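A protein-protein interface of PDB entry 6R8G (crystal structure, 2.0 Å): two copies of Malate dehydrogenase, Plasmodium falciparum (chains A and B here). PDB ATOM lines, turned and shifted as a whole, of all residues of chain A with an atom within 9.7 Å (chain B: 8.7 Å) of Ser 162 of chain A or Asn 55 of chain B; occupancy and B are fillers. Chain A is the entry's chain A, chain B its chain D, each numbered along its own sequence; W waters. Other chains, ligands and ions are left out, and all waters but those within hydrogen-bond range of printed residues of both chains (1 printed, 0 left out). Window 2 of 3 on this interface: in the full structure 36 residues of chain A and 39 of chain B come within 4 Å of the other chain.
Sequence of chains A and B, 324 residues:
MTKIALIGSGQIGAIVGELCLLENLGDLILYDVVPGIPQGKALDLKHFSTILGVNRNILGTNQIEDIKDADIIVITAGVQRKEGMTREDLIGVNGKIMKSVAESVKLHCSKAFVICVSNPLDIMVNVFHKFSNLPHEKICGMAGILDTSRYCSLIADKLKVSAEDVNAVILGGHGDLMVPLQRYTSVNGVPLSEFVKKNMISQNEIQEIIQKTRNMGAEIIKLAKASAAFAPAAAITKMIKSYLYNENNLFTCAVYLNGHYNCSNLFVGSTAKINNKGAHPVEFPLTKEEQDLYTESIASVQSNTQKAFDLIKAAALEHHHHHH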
ATOM      1  N   CYS A 152       3.501   7.116   8.158  1.00  0.00           N
ATOM      2  CA  CYS A 152       4.757   7.042   8.959  1.00  0.00           C
ATOM      3  C   CYS A 152       5.855   6.332   8.141  1.00  0.00           C
ATOM      4  O   CYS A 152       6.976   6.796   8.215  1.00  0.00           O
ATOM      5  CB  CYS A 152       4.541   6.364  10.301  1.00  0.00           C
ATOM      6  SG  CYS A 152       3.539   7.413  11.367  1.00  0.00           S
ATOM      7  N   SER A 153       5.524   5.277   7.381  1.00  0.00           N
ATOM      8  CA  SER A 153       6.477   4.554   6.519  1.00  0.00           C
ATOM      9  C   SER A 153       7.060   5.542   5.514  1.00  0.00           C
ATOM     10  O   SER A 153       8.297   5.494   5.263  1.00  0.00           O
ATOM     11  CB  SER A 153       5.842   3.438   5.746  1.00  0.00           C
ATOM     12  OG  SER A 153       5.288   2.509   6.638  1.00  0.00           O
ATOM     13  N   LEU A 154       6.191   6.332   4.883  1.00  0.00           N
ATOM     14  CA  LEU A 154       6.645   7.275   3.819  1.00  0.00           C
ATOM     15  C   LEU A 154       7.512   8.393   4.419  1.00  0.00           C
ATOM     16  O   LEU A 154       8.536   8.758   3.818  1.00  0.00           O
ATOM     17  CB  LEU A 154       5.426   7.822   3.075  1.00  0.00           C
ATOM     18  CG  LEU A 154       4.755   6.786   2.180  1.00  0.00           C
ATOM     19  CD1 LEU A 154       3.385   7.281   1.776  1.00  0.00           C
ATOM     20  CD2 LEU A 154       5.603   6.482   0.936  1.00  0.00           C
ATOM     21  N   ILE A 155       7.140   8.892   5.581  1.00  0.00           N
ATOM     22  CA  ILE A 155       7.942   9.951   6.268  1.00  0.00           C
ATOM     23  C   ILE A 155       9.306   9.332   6.621  1.00  0.00           C
ATOM     24  O   ILE A 155      10.347   9.972   6.358  1.00  0.00           O
ATOM     25  CB  ILE A 155       7.220  10.516   7.515  1.00  0.00           C
ATOM     26  CG1 ILE A 155       5.913  11.245   7.193  1.00  0.00           C
ATOM     27  CG2 ILE A 155       8.136  11.341   8.373  1.00  0.00           C
ATOM     28  CD1 ILE A 155       6.065  12.597   6.599  1.00  0.00           C
ATOM     29  N   ALA A 156       9.314   8.134   7.200  1.00  0.00           N
ATOM     30  CA  ALA A 156      10.575   7.465   7.601  1.00  0.00           C
ATOM     31  C   ALA A 156      11.480   7.257   6.366  1.00  0.00           C
ATOM     32  O   ALA A 156      12.666   7.550   6.476  1.00  0.00           O
ATOM     33  CB  ALA A 156      10.299   6.181   8.300  1.00  0.00           C
ATOM     34  N   ASP A 157      10.930   6.815   5.242  1.00  0.00           N
ATOM     35  CA  ASP A 157      11.704   6.600   3.974  1.00  0.00           C
ATOM     36  C   ASP A 157      12.393   7.897   3.566  1.00  0.00           C
ATOM     37  O   ASP A 157      13.570   7.842   3.237  1.00  0.00           O
ATOM     38  CB  ASP A 157      10.844   6.165   2.778  1.00  0.00           C
ATOM     39  CG  ASP A 157      10.322   4.731   2.853  1.00  0.00           C
ATOM     40  OD1 ASP A 157      10.861   3.938   3.658  1.00  0.00           O
ATOM     41  OD2 ASP A 157       9.345   4.416   2.131  1.00  0.00           O
ATOM     42  N   LYS A 158      11.671   9.019   3.584  1.00  0.00           N
ATOM     43  CA  LYS A 158      12.185  10.320   3.112  1.00  0.00           C
ATOM     44  C   LYS A 158      13.294  10.808   4.048  1.00  0.00           C
ATOM     45  O   LYS A 158      14.302  11.298   3.549  1.00  0.00           O
ATOM     46  CB  LYS A 158      11.043  11.339   3.047  1.00  0.00           C
ATOM     47  CG  LYS A 158       9.966  10.932   2.073  1.00  0.00           C
ATOM     48  CD  LYS A 158       8.859  12.017   1.972  1.00  0.00           C
ATOM     49  CE  LYS A 158       9.281  13.293   1.264  1.00  0.00           C
ATOM     50  NZ  LYS A 158       9.525  13.060  -0.191  1.00  0.00           N
ATOM     51  N   LEU A 159      13.128  10.658   5.364  1.00  0.00           N
ATOM     52  CA  LEU A 159      14.096  11.146   6.380  1.00  0.00           C
ATOM     53  C   LEU A 159      15.254  10.161   6.558  1.00  0.00           C
ATOM     54  O   LEU A 159      16.154  10.490   7.316  1.00  0.00           O
ATOM     55  CB  LEU A 159      13.377  11.346   7.719  1.00  0.00           C
ATOM     56  CG  LEU A 159      12.308  12.438   7.749  1.00  0.00           C
ATOM     57  CD1 LEU A 159      11.652  12.550   9.123  1.00  0.00           C
ATOM     58  CD2 LEU A 159      12.872  13.766   7.355  1.00  0.00           C
ATOM     59  N   LYS A 160      15.195   8.993   5.919  1.00  0.00           N
ATOM     60  CA  LYS A 160      16.228   7.922   5.998  1.00  0.00           C
ATOM     61  C   LYS A 160      16.400   7.493   7.461  1.00  0.00           C
ATOM     62  O   LYS A 160      17.555   7.361   7.935  1.00  0.00           O
ATOM     63  CB  LYS A 160      17.524   8.395   5.348  1.00  0.00           C
ATOM     64  CG  LYS A 160      17.442   8.596   3.837  1.00  0.00           C
ATOM     65  CD  LYS A 160      18.602   9.494   3.376  1.00  0.00           C
ATOM     66  CE  LYS A 160      18.633   9.767   1.881  1.00  0.00           C
ATOM     67  NZ  LYS A 160      19.194  11.112   1.577  1.00  0.00           N
ATOM     68  N   VAL A 161      15.276   7.233   8.136  1.00  0.00           N
ATOM     69  CA  VAL A 161      15.251   6.718   9.527  1.00  0.00           C
ATOM     70  C   VAL A 161      14.383   5.481   9.557  1.00  0.00           C
ATOM     71  O   VAL A 161      13.509   5.313   8.684  1.00  0.00           O
ATOM     72  CB  VAL A 161      14.762   7.760  10.549  1.00  0.00           C
ATOM     73  CG1 VAL A 161      15.748   8.916  10.649  1.00  0.00           C
ATOM     74  CG2 VAL A 161      13.345   8.253  10.244  1.00  0.00           C
ATOM     75  N   SER A 162      14.609   4.653  10.563  1.00  0.00           N
ATOM     76  CA  SER A 162      13.658   3.584  10.938  1.00  0.00           C
ATOM     77  C   SER A 162      12.271   4.224  11.090  1.00  0.00           C
ATOM     78  O   SER A 162      12.176   5.411  11.570  1.00  0.00           O
ATOM     79  CB  SER A 162      14.110   2.909  12.187  1.00  0.00           C
ATOM     80  OG  SER A 162      13.087   2.131  12.752  1.00  0.00           O
ATOM     81  N   ALA A 163      11.226   3.470  10.778  1.00  0.00           N
ATOM     82  CA  ALA A 163       9.827   3.827  11.115  1.00  0.00           C
ATOM     83  C   ALA A 163       9.495   3.534  12.593  1.00  0.00           C
ATOM     84  O   ALA A 163       8.506   4.037  13.035  1.00  0.00           O
ATOM     85  CB  ALA A 163       8.899   3.076  10.189  1.00  0.00           C
ATOM     86  N   GLU A 164      10.312   2.817  13.375  1.00  0.00           N
ATOM     87  CA  GLU A 164       9.887   2.317  14.713  1.00  0.00           C
ATOM     88  C   GLU A 164       9.469   3.469  15.616  1.00  0.00           C
ATOM     89  O   GLU A 164       8.657   3.247  16.462  1.00  0.00           O
ATOM     90  CB  GLU A 164      10.977   1.536  15.451  1.00  0.00           C
ATOM     91  CG  GLU A 164      11.166   0.112  14.948  1.00  0.00           C
ATOM     92  CD  GLU A 164      12.039  -0.727  15.865  1.00  0.00           C
ATOM     93  OE1 GLU A 164      12.994  -1.343  15.377  1.00  0.00           O
ATOM     94  OE2 GLU A 164      11.849  -0.657  17.066  1.00  0.00           O
ATOM     95  N   ASP A 165      10.039   4.643  15.485  1.00  0.00           N
ATOM     96  CA  ASP A 165       9.748   5.769  16.424  1.00  0.00           C
ATOM     97  C   ASP A 165       9.088   6.950  15.672  1.00  0.00           C
ATOM     98  O   ASP A 165       9.020   8.048  16.262  1.00  0.00           O
ATOM     99  CB  ASP A 165      11.006   6.165  17.215  1.00  0.00           C
ATOM    100  CG  ASP A 165      11.526   5.053  18.133  1.00  0.00           C
ATOM    101  OD1 ASP A 165      10.772   4.630  18.976  1.00  0.00           O
ATOM    102  OD2 ASP A 165      12.666   4.597  17.952  1.00  0.00           O
ATOM    103  N   VAL A 166       8.573   6.728  14.465  1.00  0.00           N
ATOM    104  CA  VAL A 166       7.744   7.742  13.743  1.00  0.00           C
ATOM    105  C   VAL A 166       6.274   7.480  14.089  1.00  0.00           C
ATOM    106  O   VAL A 166       5.779   6.389  13.863  1.00  0.00           O
ATOM    107  CB  VAL A 166       7.996   7.718  12.232  1.00  0.00           C
ATOM    108  CG1 VAL A 166       7.217   8.790  11.502  1.00  0.00           C
ATOM    109  CG2 VAL A 166       9.477   7.843  11.922  1.00  0.00           C
ATOM    110  N   ASN A 167       5.634   8.470  14.663  1.00  0.00           N
ATOM    111  CA  ASN A 167       4.280   8.381  15.214  1.00  0.00           C
ATOM    112  C   ASN A 167       3.472   9.546  14.647  1.00  0.00           C
ATOM    113  O   ASN A 167       4.042  10.618  14.488  1.00  0.00           O
ATOM    114  CB  ASN A 167       4.320   8.447  16.748  1.00  0.00           C
ATOM    115  CG  ASN A 167       4.961   7.225  17.357  1.00  0.00           C
ATOM    116  OD1 ASN A 167       6.121   7.223  17.672  1.00  0.00           O
ATOM    117  ND2 ASN A 167       4.241   6.144  17.442  1.00  0.00           N
ATOM    118  N   SER A 186       5.633  12.947  15.019  1.00  0.00           N
ATOM    119  CA  SER A 186       6.954  13.084  15.677  1.00  0.00           C
ATOM    120  C   SER A 186       7.856  11.932  15.264  1.00  0.00           C
ATOM    121  O   SER A 186       7.338  10.861  14.897  1.00  0.00           O
ATOM    122  CB  SER A 186       6.842  13.221  17.192  1.00  0.00           C
ATOM    123  OG  SER A 186       6.424  12.023  17.827  1.00  0.00           O
ATOM    124  N   VAL A 187       9.149  12.216  15.303  1.00  0.00           N
ATOM    125  CA  VAL A 187      10.252  11.269  15.035  1.00  0.00           C
ATOM    126  C   VAL A 187      11.063  11.162  16.331  1.00  0.00           C
ATOM    127  O   VAL A 187      11.878  12.073  16.651  1.00  0.00           O
ATOM    128  CB  VAL A 187      11.095  11.699  13.811  1.00  0.00           C
ATOM    129  CG1 VAL A 187      12.182  10.695  13.493  1.00  0.00           C
ATOM    130  CG2 VAL A 187      10.234  11.913  12.580  1.00  0.00           C
ATOM    131  N   ASN A 188      10.829  10.078  17.059  1.00  0.00           N
ATOM    132  CA  ASN A 188      11.405   9.821  18.386  1.00  0.00           C
ATOM    133  C   ASN A 188      11.244  11.065  19.273  1.00  0.00           C
ATOM    134  O   ASN A 188      12.208  11.486  19.909  1.00  0.00           O
ATOM    135  CB  ASN A 188      12.842   9.331  18.279  1.00  0.00           C
ATOM    136  CG  ASN A 188      13.294   8.818  19.633  1.00  0.00           C
ATOM    137  OD1 ASN A 188      12.508   8.172  20.362  1.00  0.00           O
ATOM    138  ND2 ASN A 188      14.506   9.215  19.995  1.00  0.00           N
ATOM    139  N   PHE A 195      12.110  18.905  11.246  1.00  0.00           N
ATOM    140  CA  PHE A 195      12.722  18.288  10.037  1.00  0.00           C
ATOM    141  C   PHE A 195      12.499  19.220   8.838  1.00  0.00           C
ATOM    142  O   PHE A 195      13.415  19.351   8.003  1.00  0.00           O
ATOM    143  CB  PHE A 195      12.184  16.880   9.810  1.00  0.00           C
ATOM    144  CG  PHE A 195      12.587  15.957  10.912  1.00  0.00           C
ATOM    145  CD1 PHE A 195      13.795  15.286  10.835  1.00  0.00           C
ATOM    146  CD2 PHE A 195      11.830  15.863  12.067  1.00  0.00           C
ATOM    147  CE1 PHE A 195      14.176  14.425  11.846  1.00  0.00           C
ATOM    148  CE2 PHE A 195      12.223  15.019  13.092  1.00  0.00           C
ATOM    149  CZ  PHE A 195      13.400  14.316  12.990  1.00  0.00           C
ATOM    150  N   LEU B  21      10.060 -11.606   7.269  1.00  0.00           N
ATOM    151  CA  LEU B  21      10.041 -10.288   7.937  1.00  0.00           C
ATOM    152  C   LEU B  21       9.798 -10.469   9.440  1.00  0.00           C
ATOM    153  O   LEU B  21      10.521  -9.879  10.173  1.00  0.00           O
ATOM    154  CB  LEU B  21       8.991  -9.387   7.274  1.00  0.00           C
ATOM    155  CG  LEU B  21       9.269  -9.002   5.824  1.00  0.00           C
ATOM    156  CD1 LEU B  21       8.003  -8.467   5.187  1.00  0.00           C
ATOM    157  CD2 LEU B  21      10.393  -7.986   5.697  1.00  0.00           C
ATOM    158  N   LEU B  22       8.818 -11.250   9.858  1.00  0.00           N
ATOM    159  CA  LEU B  22       8.565 -11.517  11.295  1.00  0.00           C
ATOM    160  C   LEU B  22       9.814 -12.106  11.973  1.00  0.00           C
ATOM    161  O   LEU B  22      10.092 -11.743  13.096  1.00  0.00           O
ATOM    162  CB  LEU B  22       7.386 -12.468  11.439  1.00  0.00           C
ATOM    163  CG  LEU B  22       6.034 -11.793  11.233  1.00  0.00           C
ATOM    164  CD1 LEU B  22       4.914 -12.821  11.067  1.00  0.00           C
ATOM    165  CD2 LEU B  22       5.731 -10.797  12.363  1.00  0.00           C
ATOM    166  N   ASN B  24      12.821 -11.647  10.996  1.00  0.00           N
ATOM    167  CA  ASN B  24      13.943 -10.747  10.653  1.00  0.00           C
ATOM    168  C   ASN B  24      15.083 -11.450   9.886  1.00  0.00           C
ATOM    169  O   ASN B  24      16.232 -11.053  10.104  1.00  0.00           O
ATOM    170  CB  ASN B  24      14.523 -10.099  11.911  1.00  0.00           C
ATOM    171  CG  ASN B  24      14.526  -8.595  11.818  1.00  0.00           C
ATOM    172  OD1 ASN B  24      14.672  -8.021  10.753  1.00  0.00           O
ATOM    173  ND2 ASN B  24      14.166  -7.947  12.900  1.00  0.00           N
ATOM    174  N   GLY B  26      15.976 -11.310   6.618  1.00  0.00           N
ATOM    175  CA  GLY B  26      16.655 -10.582   5.535  1.00  0.00           C
ATOM    176  C   GLY B  26      15.769  -9.571   4.844  1.00  0.00           C
ATOM    177  O   GLY B  26      14.569  -9.487   5.161  1.00  0.00           O
ATOM    178  N   ASP B  27      16.379  -8.858   3.911  1.00  0.00           N
ATOM    179  CA  ASP B  27      15.695  -8.002   2.931  1.00  0.00           C
ATOM    180  C   ASP B  27      15.011  -8.930   1.935  1.00  0.00           C
ATOM    181  O   ASP B  27      15.535 -10.024   1.710  1.00  0.00           O
ATOM    182  CB  ASP B  27      16.696  -7.061   2.270  1.00  0.00           C
ATOM    183  CG  ASP B  27      17.294  -6.061   3.220  1.00  0.00           C
ATOM    184  OD1 ASP B  27      16.634  -5.700   4.204  1.00  0.00           O
ATOM    185  OD2 ASP B  27      18.395  -5.626   2.943  1.00  0.00           O
ATOM    186  N   LEU B  28      13.895  -8.488   1.373  1.00  0.00           N
ATOM    187  CA  LEU B  28      13.113  -9.263   0.403  1.00  0.00           C
ATOM    188  C   LEU B  28      13.219  -8.637  -0.986  1.00  0.00           C
ATOM    189  O   LEU B  28      13.125  -7.413  -1.145  1.00  0.00           O
ATOM    190  CB  LEU B  28      11.640  -9.294   0.794  1.00  0.00           C
ATOM    191  CG  LEU B  28      11.318  -9.938   2.136  1.00  0.00           C
ATOM    192  CD1 LEU B  28       9.808  -9.985   2.321  1.00  0.00           C
ATOM    193  CD2 LEU B  28      11.879 -11.346   2.217  1.00  0.00           C
ATOM    194  N   LEU B  45       3.394  -5.403   2.449  1.00  0.00           N
ATOM    195  CA  LEU B  45       4.391  -5.962   3.397  1.00  0.00           C
ATOM    196  C   LEU B  45       5.232  -4.845   4.031  1.00  0.00           C
ATOM    197  O   LEU B  45       5.596  -5.004   5.209  1.00  0.00           O
ATOM    198  CB  LEU B  45       5.183  -7.067   2.724  1.00  0.00           C
ATOM    199  CG  LEU B  45       4.380  -8.353   2.469  1.00  0.00           C
ATOM    200  CD1 LEU B  45       5.151  -9.313   1.617  1.00  0.00           C
ATOM    201  CD2 LEU B  45       3.952  -9.033   3.741  1.00  0.00           C
ATOM    202  N   LYS B  46       5.476  -3.735   3.335  1.00  0.00           N
ATOM    203  CA  LYS B  46       6.149  -2.557   3.950  1.00  0.00           C
ATOM    204  C   LYS B  46       5.221  -2.021   5.058  1.00  0.00           C
ATOM    205  O   LYS B  46       5.733  -1.704   6.124  1.00  0.00           O
ATOM    206  CB  LYS B  46       6.456  -1.414   2.966  1.00  0.00           C
ATOM    207  CG  LYS B  46       7.642  -1.666   2.029  1.00  0.00           C
ATOM    208  CD  LYS B  46       8.125  -0.508   1.123  1.00  0.00           C
ATOM    209  CE  LYS B  46       8.550  -0.938  -0.277  1.00  0.00           C
ATOM    210  NZ  LYS B  46       7.552  -0.504  -1.314  1.00  0.00           N
ATOM    211  N   PHE B  48       2.840  -3.555   6.753  1.00  0.00           N
ATOM    212  CA  PHE B  48       2.820  -4.638   7.745  1.00  0.00           C
ATOM    213  C   PHE B  48       4.070  -4.499   8.623  1.00  0.00           C
ATOM    214  O   PHE B  48       3.917  -4.511   9.879  1.00  0.00           O
ATOM    215  CB  PHE B  48       2.789  -5.968   6.992  1.00  0.00           C
ATOM    216  CG  PHE B  48       3.080  -7.193   7.802  1.00  0.00           C
ATOM    217  CD1 PHE B  48       2.054  -7.889   8.430  1.00  0.00           C
ATOM    218  CD2 PHE B  48       4.355  -7.694   7.887  1.00  0.00           C
ATOM    219  CE1 PHE B  48       2.318  -9.009   9.193  1.00  0.00           C
ATOM    220  CE2 PHE B  48       4.616  -8.814   8.657  1.00  0.00           C
ATOM    221  CZ  PHE B  48       3.596  -9.490   9.269  1.00  0.00           C
ATOM    222  N   SER B  49       5.244  -4.330   7.987  1.00  0.00           N
ATOM    223  CA  SER B  49       6.542  -4.147   8.682  1.00  0.00           C
ATOM    224  C   SER B  49       6.478  -2.986   9.661  1.00  0.00           C
ATOM    225  O   SER B  49       6.943  -3.155  10.811  1.00  0.00           O
ATOM    226  CB  SER B  49       7.678  -3.993   7.707  1.00  0.00           C
ATOM    227  OG  SER B  49       7.801  -5.215   7.012  1.00  0.00           O
ATOM    228  N   THR B  50       5.940  -1.845   9.236  1.00  0.00           N
ATOM    229  CA  THR B  50       5.889  -0.627  10.045  1.00  0.00           C
ATOM    230  C   THR B  50       5.025  -0.892  11.273  1.00  0.00           C
ATOM    231  O   THR B  50       5.418  -0.481  12.365  1.00  0.00           O
ATOM    232  CB  THR B  50       5.337   0.537   9.240  1.00  0.00           C
ATOM    233  OG1 THR B  50       6.242   0.761   8.168  1.00  0.00           O
ATOM    234  CG2 THR B  50       5.167   1.769  10.075  1.00  0.00           C
ATOM    235  N   ILE B  51       3.901  -1.573  11.109  1.00  0.00           N
ATOM    236  CA  ILE B  51       2.990  -1.833  12.245  1.00  0.00           C
ATOM    237  C   ILE B  51       3.707  -2.795  13.193  1.00  0.00           C
ATOM    238  O   ILE B  51       3.559  -2.620  14.343  1.00  0.00           O
ATOM    239  CB  ILE B  51       1.643  -2.405  11.789  1.00  0.00           C
ATOM    240  CG1 ILE B  51       0.918  -1.420  10.871  1.00  0.00           C
ATOM    241  CG2 ILE B  51       0.812  -2.827  13.001  1.00  0.00           C
ATOM    242  CD1 ILE B  51      -0.201  -2.052  10.057  1.00  0.00           C
ATOM    243  N   LEU B  52       4.453  -3.783  12.696  1.00  0.00           N
ATOM    244  CA  LEU B  52       5.060  -4.785  13.605  1.00  0.00           C
ATOM    245  C   LEU B  52       6.495  -4.409  14.030  1.00  0.00           C
ATOM    246  O   LEU B  52       7.033  -5.168  14.724  1.00  0.00           O
ATOM    247  CB  LEU B  52       4.955  -6.151  12.931  1.00  0.00           C
ATOM    248  CG  LEU B  52       3.489  -6.543  12.714  1.00  0.00           C
ATOM    249  CD1 LEU B  52       3.339  -7.948  12.238  1.00  0.00           C
ATOM    250  CD2 LEU B  52       2.640  -6.335  13.973  1.00  0.00           C
ATOM    251  N   GLY B  53       7.070  -3.278  13.643  1.00  0.00           N
ATOM    252  CA  GLY B  53       8.419  -2.863  14.054  1.00  0.00           C
ATOM    253  C   GLY B  53       9.534  -3.626  13.358  1.00  0.00           C
ATOM    254  O   GLY B  53      10.594  -3.691  13.908  1.00  0.00           O
ATOM    255  N   VAL B  54       9.334  -4.123  12.153  1.00  0.00           N
ATOM    256  CA  VAL B  54      10.388  -4.711  11.277  1.00  0.00           C
ATOM    257  C   VAL B  54      10.926  -3.660  10.299  1.00  0.00           C
ATOM    258  O   VAL B  54      10.146  -2.890   9.812  1.00  0.00           O
ATOM    259  CB  VAL B  54       9.840  -5.886  10.476  1.00  0.00           C
ATOM    260  CG1 VAL B  54      10.960  -6.564   9.732  1.00  0.00           C
ATOM    261  CG2 VAL B  54       9.018  -6.853  11.315  1.00  0.00           C
ATOM    262  N   ASN B  55      12.217  -3.678   9.988  1.00  0.00           N
ATOM    263  CA  ASN B  55      12.982  -2.558   9.372  1.00  0.00           C
ATOM    264  C   ASN B  55      13.713  -3.019   8.107  1.00  0.00           C
ATOM    265  O   ASN B  55      14.600  -2.370   7.631  1.00  0.00           O
ATOM    266  CB  ASN B  55      13.973  -1.965  10.383  1.00  0.00           C
ATOM    267  CG  ASN B  55      13.259  -1.471  11.627  1.00  0.00           C
ATOM    268  OD1 ASN B  55      12.385  -0.590  11.554  1.00  0.00           O
ATOM    269  ND2 ASN B  55      13.566  -2.128  12.734  1.00  0.00           N
ATOM    270  N   ARG B  56      13.362  -4.152   7.548  1.00  0.00           N
ATOM    271  CA  ARG B  56      14.017  -4.704   6.344  1.00  0.00           C
ATOM    272  C   ARG B  56      13.504  -4.026   5.067  1.00  0.00           C
ATOM    273  O   ARG B  56      12.361  -3.603   4.997  1.00  0.00           O
ATOM    274  CB  ARG B  56      13.745  -6.207   6.313  1.00  0.00           C
ATOM    275  CG  ARG B  56      14.302  -6.958   7.521  1.00  0.00           C
ATOM    276  CD  ARG B  56      15.782  -6.808   7.612  1.00  0.00           C
ATOM    277  NE  ARG B  56      16.350  -7.882   8.390  1.00  0.00           N
ATOM    278  CZ  ARG B  56      17.632  -8.275   8.338  1.00  0.00           C
ATOM    279  NH1 ARG B  56      18.519  -7.648   7.583  1.00  0.00           N
ATOM    280  NH2 ARG B  56      18.020  -9.302   9.071  1.00  0.00           N
ATOM    281  N   ASN B  57      14.336  -3.977   4.038  1.00  0.00           N
ATOM    282  CA  ASN B  57      13.953  -3.508   2.689  1.00  0.00           C
ATOM    283  C   ASN B  57      13.067  -4.558   2.023  1.00  0.00           C
ATOM    284  O   ASN B  57      13.333  -5.772   2.234  1.00  0.00           O
ATOM    285  CB  ASN B  57      15.197  -3.245   1.851  1.00  0.00           C
ATOM    286  CG  ASN B  57      15.929  -2.042   2.361  1.00  0.00           C
ATOM    287  OD1 ASN B  57      15.318  -0.980   2.503  1.00  0.00           O
ATOM    288  ND2 ASN B  57      17.218  -2.199   2.596  1.00  0.00           N
ATOM    289  N   ILE B  58      12.065  -4.119   1.269  1.00  0.00           N
ATOM    290  CA  ILE B  58      11.184  -4.976   0.444  1.00  0.00           C
ATOM    291  C   ILE B  58      11.083  -4.361  -0.948  1.00  0.00           C
ATOM    292  O   ILE B  58      10.681  -3.223  -1.030  1.00  0.00           O
ATOM    293  CB  ILE B  58       9.796  -5.123   1.085  1.00  0.00           C
ATOM    294  CG1 ILE B  58       9.941  -5.601   2.536  1.00  0.00           C
ATOM    295  CG2 ILE B  58       8.979  -6.064   0.233  1.00  0.00           C
ATOM    296  CD1 ILE B  58       8.810  -5.280   3.431  1.00  0.00           C
HETATM  297  O   HOH W   1      11.731   0.918   9.587  1.00  0.00           O
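The side-chain hydroxyl (OG1) of Thr 50 of chain B sits at hydrogen-bond distance from the side-chain hydroxyl (OG) of Ser 153 of chain A, 2.5 Å away.
The side-chain hydroxyl (OG) of Ser 162 of chain A is in hydrogen-bond range of the side-chain amide oxygen (OD1) of Asn 55 of chain B, 3.1 Å away.
The side-chain amide nitrogen of Asn 55 of chain B is in hydrogen-bond range of the side-chain carboxylate of Glu 164 of chain A.
The side-chain hydroxyl (OG) of Ser 162 of chain A lies within hydrogen-bond range of the backbone NH (N) of Glu 164 of chain A, at 2.9 Å.
The side-chain hydroxyl (OG1) of Thr 50 of chain B sits at hydrogen-bond distance from the backbone carbonyl oxygen (O) of Lys 46 of chain B.
Ala 163 of chain A touches Thr 50 of chain B.
O of Gly 53 of chain B touches OE1 of Glu 164 of chain A (3.7 Å).
Of chain B, only Asn 55 (3.1 Å) comes within 4 Å of Ser 162 of chain A.
Of chain A, only Ser 162 and Glu 164 come within 4 Å of Asn 55 of chain B.
Printed residues of chain B within 4 Å of Ala 163 of chain A: Thr 50.
No residue of chain A comes within 4 Å of Val 54 of chain B.
Of the printed residues of chain A, Gly 53 of chain B touches Glu 164.
Printed residues of chain A within 4 Å of Thr 50 of chain B: Ser 153 and Ala 163.
Of the printed residues of chain B, Glu 164 of chain A touches Gly 53 and Asn 55.
Of the printed residues of chain B, Ser 153 of chain A touches Thr 50.
Leu 154 of chain A touches none of the printed residues of chain B.
Asn 57 of chain B touches none of the printed residues of chain A.
The nearest residue of chain A that does not touch Asn 55 of chain B is Ala 163 of chain A (4.3 Å).
The nearest printed residue of chain A that does not touch Gly 53 of chain B is Ser 162 of chain A (6.4 Å).
Printed residues of chain B that touch a printed residue of chain A: Thr 50, Gly 53 and Asn 55.
No position is printed for both chains.
Of the 5 pairs that touch across the chains among the printed residues, none has its exchanged pair printed and touching as well.
Water W1 bridges the side-chain amide oxygen of Asn 55 of chain B (2.6 Å) and the backbone NH of Ala 163 of chain A (2.9 Å).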
